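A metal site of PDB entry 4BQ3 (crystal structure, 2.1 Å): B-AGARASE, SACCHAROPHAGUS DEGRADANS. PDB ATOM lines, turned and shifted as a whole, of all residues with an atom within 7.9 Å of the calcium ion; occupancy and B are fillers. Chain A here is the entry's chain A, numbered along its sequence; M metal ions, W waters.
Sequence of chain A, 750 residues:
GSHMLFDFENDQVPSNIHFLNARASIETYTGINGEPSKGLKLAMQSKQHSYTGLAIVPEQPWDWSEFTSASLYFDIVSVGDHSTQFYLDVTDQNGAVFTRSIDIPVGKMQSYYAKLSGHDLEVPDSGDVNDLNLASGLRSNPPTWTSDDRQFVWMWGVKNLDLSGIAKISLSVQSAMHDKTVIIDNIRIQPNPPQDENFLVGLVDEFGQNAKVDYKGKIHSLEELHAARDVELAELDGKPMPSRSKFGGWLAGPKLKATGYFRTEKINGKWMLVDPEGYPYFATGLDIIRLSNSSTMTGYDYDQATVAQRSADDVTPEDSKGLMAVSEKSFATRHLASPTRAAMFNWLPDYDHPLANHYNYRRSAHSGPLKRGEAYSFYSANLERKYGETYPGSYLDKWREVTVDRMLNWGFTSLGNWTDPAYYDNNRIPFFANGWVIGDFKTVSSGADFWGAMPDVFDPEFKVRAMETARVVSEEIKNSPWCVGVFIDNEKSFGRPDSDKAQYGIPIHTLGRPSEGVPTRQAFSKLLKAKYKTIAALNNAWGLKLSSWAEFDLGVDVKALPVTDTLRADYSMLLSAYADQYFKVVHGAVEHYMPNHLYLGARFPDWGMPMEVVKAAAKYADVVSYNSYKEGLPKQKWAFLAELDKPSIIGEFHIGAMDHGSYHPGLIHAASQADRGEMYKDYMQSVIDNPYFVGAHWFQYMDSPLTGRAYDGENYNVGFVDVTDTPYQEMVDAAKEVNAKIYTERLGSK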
ATOM      1  N   MET A   4     -19.353   4.934  10.706  1.00  0.00           N
ATOM      2  CA  MET A   4     -18.168   4.192  10.251  1.00  0.00           C
ATOM      3  C   MET A   4     -18.242   2.785  10.827  1.00  0.00           C
ATOM      4  O   MET A   4     -18.384   2.621  12.033  1.00  0.00           O
ATOM      5  CB  MET A   4     -16.866   4.843  10.741  1.00  0.00           C
ATOM      6  CG  MET A   4     -15.608   4.089  10.280  1.00  0.00           C
ATOM      7  SD  MET A   4     -15.499   4.107   8.460  1.00  0.00           S
ATOM      8  CE  MET A   4     -15.159   5.843   8.124  1.00  0.00           C
ATOM      9  N   PHE A   6     -15.895   0.100   9.437  1.00  0.00           N
ATOM     10  CA  PHE A   6     -14.496  -0.390   9.393  1.00  0.00           C
ATOM     11  C   PHE A   6     -13.593   0.629   8.662  1.00  0.00           C
ATOM     12  O   PHE A   6     -13.742   0.872   7.444  1.00  0.00           O
ATOM     13  CB  PHE A   6     -14.388  -1.783   8.732  1.00  0.00           C
ATOM     14  CG  PHE A   6     -15.145  -2.888   9.436  1.00  0.00           C
ATOM     15  CD1 PHE A   6     -14.619  -3.504  10.571  1.00  0.00           C
ATOM     16  CD2 PHE A   6     -16.367  -3.341   8.934  1.00  0.00           C
ATOM     17  CE1 PHE A   6     -15.309  -4.541  11.219  1.00  0.00           C
ATOM     18  CE2 PHE A   6     -17.059  -4.390   9.569  1.00  0.00           C
ATOM     19  CZ  PHE A   6     -16.527  -4.983  10.728  1.00  0.00           C
ATOM     20  N   ASP A   7     -12.687   1.249   9.415  1.00  0.00           N
ATOM     21  CA  ASP A   7     -11.714   2.168   8.810  1.00  0.00           C
ATOM     22  C   ASP A   7     -10.318   1.575   8.873  1.00  0.00           C
ATOM     23  O   ASP A   7      -9.374   2.135   8.302  1.00  0.00           O
ATOM     24  CB  ASP A   7     -11.789   3.567   9.409  1.00  0.00           C
ATOM     25  CG  ASP A   7     -11.292   3.659  10.857  1.00  0.00           C
ATOM     26  OD1 ASP A   7     -10.622   2.739  11.413  1.00  0.00           O
ATOM     27  OD2 ASP A   7     -11.565   4.715  11.432  1.00  0.00           O
ATOM     28  N   PHE A   8     -10.221   0.401   9.510  1.00  0.00           N
ATOM     29  CA  PHE A   8      -8.941  -0.346   9.650  1.00  0.00           C
ATOM     30  C   PHE A   8      -7.807   0.427  10.323  1.00  0.00           C
ATOM     31  O   PHE A   8      -6.661  -0.022  10.343  1.00  0.00           O
ATOM     32  CB  PHE A   8      -8.533  -0.949   8.290  1.00  0.00           C
ATOM     33  CG  PHE A   8      -9.661  -1.722   7.647  1.00  0.00           C
ATOM     34  CD1 PHE A   8     -10.023  -2.966   8.146  1.00  0.00           C
ATOM     35  CD2 PHE A   8     -10.424  -1.152   6.630  1.00  0.00           C
ATOM     36  CE1 PHE A   8     -11.104  -3.669   7.619  1.00  0.00           C
ATOM     37  CE2 PHE A   8     -11.506  -1.831   6.098  1.00  0.00           C
ATOM     38  CZ  PHE A   8     -11.846  -3.104   6.578  1.00  0.00           C
ATOM     39  N   GLU A   9      -8.126   1.566  10.929  1.00  0.00           N
ATOM     40  CA  GLU A   9      -7.071   2.364  11.500  1.00  0.00           C
ATOM     41  C   GLU A   9      -6.436   1.726  12.734  1.00  0.00           C
ATOM     42  O   GLU A   9      -5.326   2.063  13.076  1.00  0.00           O
ATOM     43  CB  GLU A   9      -7.504   3.836  11.728  1.00  0.00           C
ATOM     44  CG  GLU A   9      -7.708   4.631  10.436  1.00  0.00           C
ATOM     45  CD  GLU A   9      -6.431   4.715   9.621  1.00  0.00           C
ATOM     46  OE1 GLU A   9      -5.342   4.976  10.200  1.00  0.00           O
ATOM     47  OE2 GLU A   9      -6.492   4.421   8.404  1.00  0.00           O
ATOM     48  N   ASN A  10      -7.106   0.776  13.400  1.00  0.00           N
ATOM     49  CA  ASN A  10      -6.469   0.056  14.477  1.00  0.00           C
ATOM     50  C   ASN A  10      -5.558  -1.055  13.977  1.00  0.00           C
ATOM     51  O   ASN A  10      -5.122  -1.902  14.754  1.00  0.00           O
ATOM     52  CB  ASN A  10      -7.499  -0.524  15.460  1.00  0.00           C
ATOM     53  CG  ASN A  10      -8.399  -1.587  14.819  1.00  0.00           C
ATOM     54  OD1 ASN A  10      -8.111  -2.078  13.721  1.00  0.00           O
ATOM     55  ND2 ASN A  10      -9.474  -1.974  15.509  1.00  0.00           N
ATOM     56  N   ILE A  26      -3.677  -5.829   6.540  1.00  0.00           N
ATOM     57  CA  ILE A  26      -3.800  -4.376   6.599  1.00  0.00           C
ATOM     58  C   ILE A  26      -2.569  -3.727   6.019  1.00  0.00           C
ATOM     59  O   ILE A  26      -1.491  -4.043   6.437  1.00  0.00           O
ATOM     60  CB  ILE A  26      -3.967  -3.892   8.046  1.00  0.00           C
ATOM     61  CG1 ILE A  26      -5.144  -4.647   8.714  1.00  0.00           C
ATOM     62  CG2 ILE A  26      -4.136  -2.367   8.064  1.00  0.00           C
ATOM     63  CD1 ILE A  26      -6.450  -4.593   7.936  1.00  0.00           C
ATOM     64  N   GLU A  27      -2.740  -2.826   5.054  1.00  0.00           N
ATOM     65  CA  GLU A  27      -1.599  -2.202   4.390  1.00  0.00           C
ATOM     66  C   GLU A  27      -1.887  -0.741   4.262  1.00  0.00           C
ATOM     67  O   GLU A  27      -3.037  -0.363   4.045  1.00  0.00           O
ATOM     68  CB  GLU A  27      -1.368  -2.726   2.957  1.00  0.00           C
ATOM     69  CG  GLU A  27      -1.267  -4.248   2.815  1.00  0.00           C
ATOM     70  CD  GLU A  27      -0.021  -4.867   3.472  1.00  0.00           C
ATOM     71  OE1 GLU A  27       0.935  -4.138   3.852  1.00  0.00           O
ATOM     72  OE2 GLU A  27       0.006  -6.109   3.625  1.00  0.00           O
ATOM     73  N   TYR A  29      -1.968   2.417   2.164  1.00  0.00           N
ATOM     74  CA  TYR A  29      -2.129   2.748   0.751  1.00  0.00           C
ATOM     75  C   TYR A  29      -2.557   4.226   0.690  1.00  0.00           C
ATOM     76  O   TYR A  29      -2.840   4.826   1.739  1.00  0.00           O
ATOM     77  CB  TYR A  29      -3.240   1.898   0.152  1.00  0.00           C
ATOM     78  CG  TYR A  29      -4.603   2.413   0.551  1.00  0.00           C
ATOM     79  CD1 TYR A  29      -5.075   2.299   1.886  1.00  0.00           C
ATOM     80  CD2 TYR A  29      -5.417   3.063  -0.377  1.00  0.00           C
ATOM     81  CE1 TYR A  29      -6.316   2.791   2.260  1.00  0.00           C
ATOM     82  CE2 TYR A  29      -6.644   3.584   0.007  1.00  0.00           C
ATOM     83  CZ  TYR A  29      -7.085   3.436   1.319  1.00  0.00           C
ATOM     84  OH  TYR A  29      -8.300   3.954   1.662  1.00  0.00           O
ATOM     85  N   PRO A  36      -1.993   8.848   2.659  1.00  0.00           N
ATOM     86  CA  PRO A  36      -1.800   7.448   3.058  1.00  0.00           C
ATOM     87  C   PRO A  36      -2.794   7.126   4.168  1.00  0.00           C
ATOM     88  O   PRO A  36      -3.052   7.970   5.013  1.00  0.00           O
ATOM     89  CB  PRO A  36      -0.383   7.411   3.607  1.00  0.00           C
ATOM     90  CG  PRO A  36       0.279   8.674   3.172  1.00  0.00           C
ATOM     91  CD  PRO A  36      -0.762   9.642   2.708  1.00  0.00           C
ATOM     92  N   SER A  37      -3.366   5.924   4.153  1.00  0.00           N
ATOM     93  CA  SER A  37      -4.303   5.483   5.184  1.00  0.00           C
ATOM     94  C   SER A  37      -4.193   3.935   5.332  1.00  0.00           C
ATOM     95  O   SER A  37      -3.629   3.269   4.430  1.00  0.00           O
ATOM     96  CB  SER A  37      -5.706   5.933   4.748  1.00  0.00           C
ATOM     97  OG  SER A  37      -6.718   5.349   5.514  1.00  0.00           O
ATOM     98  N   LYS A  38      -4.687   3.362   6.445  1.00  0.00           N
ATOM     99  CA  LYS A  38      -4.710   1.903   6.532  1.00  0.00           C
ATOM    100  C   LYS A  38      -5.974   1.387   5.808  1.00  0.00           C
ATOM    101  O   LYS A  38      -7.068   1.900   6.063  1.00  0.00           O
ATOM    102  CB  LYS A  38      -4.740   1.390   7.986  1.00  0.00           C
ATOM    103  CG  LYS A  38      -3.532   1.711   8.860  1.00  0.00           C
ATOM    104  CD  LYS A  38      -2.222   1.475   8.145  1.00  0.00           C
ATOM    105  CE  LYS A  38      -1.049   1.404   9.140  1.00  0.00           C
ATOM    106  NZ  LYS A  38      -1.296   2.223  10.378  1.00  0.00           N
ATOM    107  N   GLY A  39      -5.812   0.388   4.948  1.00  0.00           N
ATOM    108  CA  GLY A  39      -6.963  -0.317   4.343  1.00  0.00           C
ATOM    109  C   GLY A  39      -6.778  -1.846   4.373  1.00  0.00           C
ATOM    110  O   GLY A  39      -5.720  -2.350   4.717  1.00  0.00           O
ATOM    111  N   LEU A  40      -7.829  -2.583   4.009  1.00  0.00           N
ATOM    112  CA  LEU A  40      -7.809  -4.034   4.005  1.00  0.00           C
ATOM    113  C   LEU A  40      -7.470  -4.429   2.611  1.00  0.00           C
ATOM    114  O   LEU A  40      -8.238  -4.125   1.645  1.00  0.00           O
ATOM    115  CB  LEU A  40      -9.159  -4.605   4.412  1.00  0.00           C
ATOM    116  CG  LEU A  40      -9.257  -6.123   4.412  1.00  0.00           C
ATOM    117  CD1 LEU A  40      -8.628  -6.657   5.670  1.00  0.00           C
ATOM    118  CD2 LEU A  40     -10.691  -6.580   4.368  1.00  0.00           C
ATOM    119  N   ASP A  75     -14.766   2.253   0.127  1.00  0.00           N
ATOM    120  CA  ASP A  75     -13.765   2.804  -0.765  1.00  0.00           C
ATOM    121  C   ASP A  75     -13.026   1.553  -1.260  1.00  0.00           C
ATOM    122  O   ASP A  75     -12.603   0.742  -0.457  1.00  0.00           O
ATOM    123  CB  ASP A  75     -12.779   3.738  -0.047  1.00  0.00           C
ATOM    124  CG  ASP A  75     -13.438   5.007   0.525  1.00  0.00           C
ATOM    125  OD1 ASP A  75     -14.617   5.302   0.271  1.00  0.00           O
ATOM    126  OD2 ASP A  75     -12.708   5.737   1.256  1.00  0.00           O
ATOM    127  N   ILE A 184      -9.585  -2.174   0.260  1.00  0.00           N
ATOM    128  CA  ILE A 184     -10.902  -1.677   0.664  1.00  0.00           C
ATOM    129  C   ILE A 184     -10.721  -0.877   1.945  1.00  0.00           C
ATOM    130  O   ILE A 184      -9.964  -1.301   2.859  1.00  0.00           O
ATOM    131  CB  ILE A 184     -11.874  -2.850   0.984  1.00  0.00           C
ATOM    132  CG1 ILE A 184     -12.180  -3.663  -0.279  1.00  0.00           C
ATOM    133  CG2 ILE A 184     -13.201  -2.364   1.611  1.00  0.00           C
ATOM    134  CD1 ILE A 184     -12.497  -5.151   0.051  1.00  0.00           C
ATOM    135  N   ASP A 185     -11.434   0.243   2.042  1.00  0.00           N
ATOM    136  CA  ASP A 185     -11.342   1.111   3.224  1.00  0.00           C
ATOM    137  C   ASP A 185     -12.708   1.736   3.543  1.00  0.00           C
ATOM    138  O   ASP A 185     -13.642   1.734   2.705  1.00  0.00           O
ATOM    139  CB  ASP A 185     -10.331   2.241   2.943  1.00  0.00           C
ATOM    140  CG  ASP A 185      -9.714   2.784   4.226  1.00  0.00           C
ATOM    141  OD1 ASP A 185     -10.101   2.349   5.368  1.00  0.00           O
ATOM    142  OD2 ASP A 185      -8.820   3.659   4.070  1.00  0.00           O
ATOM    143  N   ASN A 186     -12.805   2.306   4.729  1.00  0.00           N
ATOM    144  CA  ASN A 186     -13.925   3.188   5.109  1.00  0.00           C
ATOM    145  C   ASN A 186     -15.291   2.559   4.831  1.00  0.00           C
ATOM    146  O   ASN A 186     -16.114   3.141   4.148  1.00  0.00           O
ATOM    147  CB  ASN A 186     -13.747   4.565   4.448  1.00  0.00           C
ATOM    148  CG  ASN A 186     -12.419   5.223   4.845  1.00  0.00           C
ATOM    149  OD1 ASN A 186     -12.094   5.260   6.040  1.00  0.00           O
ATOM    150  ND2 ASN A 186     -11.644   5.715   3.853  1.00  0.00           N
ATOM    151  N   ILE A 187     -15.508   1.356   5.353  1.00  0.00           N
ATOM    152  CA  ILE A 187     -16.778   0.688   5.154  1.00  0.00           C
ATOM    153  C   ILE A 187     -17.756   1.353   6.116  1.00  0.00           C
ATOM    154  O   ILE A 187     -17.520   1.376   7.321  1.00  0.00           O
ATOM    155  CB  ILE A 187     -16.693  -0.827   5.437  1.00  0.00           C
ATOM    156  CG1 ILE A 187     -15.674  -1.495   4.476  1.00  0.00           C
ATOM    157  CG2 ILE A 187     -18.055  -1.482   5.255  1.00  0.00           C
ATOM    158  CD1 ILE A 187     -15.434  -2.968   4.731  1.00  0.00           C
HETATM  159 CA    CA M   1      -8.370   3.586   6.823  1.00  0.00          CA
HETATM  160  O   HOH W   1      -9.703   5.476   7.090  1.00  0.00           O
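OD2 of Asp 185 sits close to OH of Tyr 29 (2.5 Å).
The side-chain amide nitrogen (ND2) of Asn 186 lies close to the side-chain carboxylate (OD2) of Asp 185 (3.5 Å).
The backbone NH (N) of Ser 37 lies within hydrogen-bond range of the backbone carbonyl oxygen (O) of Tyr 29 (2.7 Å).
N of Asp 185 is in hydrogen-bond range of O of Asp 75 (2.8 Å).
Within 4 Å of the calcium ion: Asp 7, Glu 9, Ser 37, Lys 38 and Asp 185.
The calcium ion is bound by the backbone carbonyl oxygen (O) of Lys 38 (2.3 Å), the backbone carbonyl oxygen (O) of Asp 7 (2.3 Å), water W1 (2.3 Å), the side-chain carboxylate (OD1) of Asp 185 (2.6 Å), the side-chain carboxylate (OE2) of Glu 9 (2.6 Å), the side-chain hydroxyl (OG) of Ser 37 (2.7 Å) and the side-chain carboxylate (OD2) of Asp 185 (2.8 Å).
The calcium ion has seven donor atoms within binding distance.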
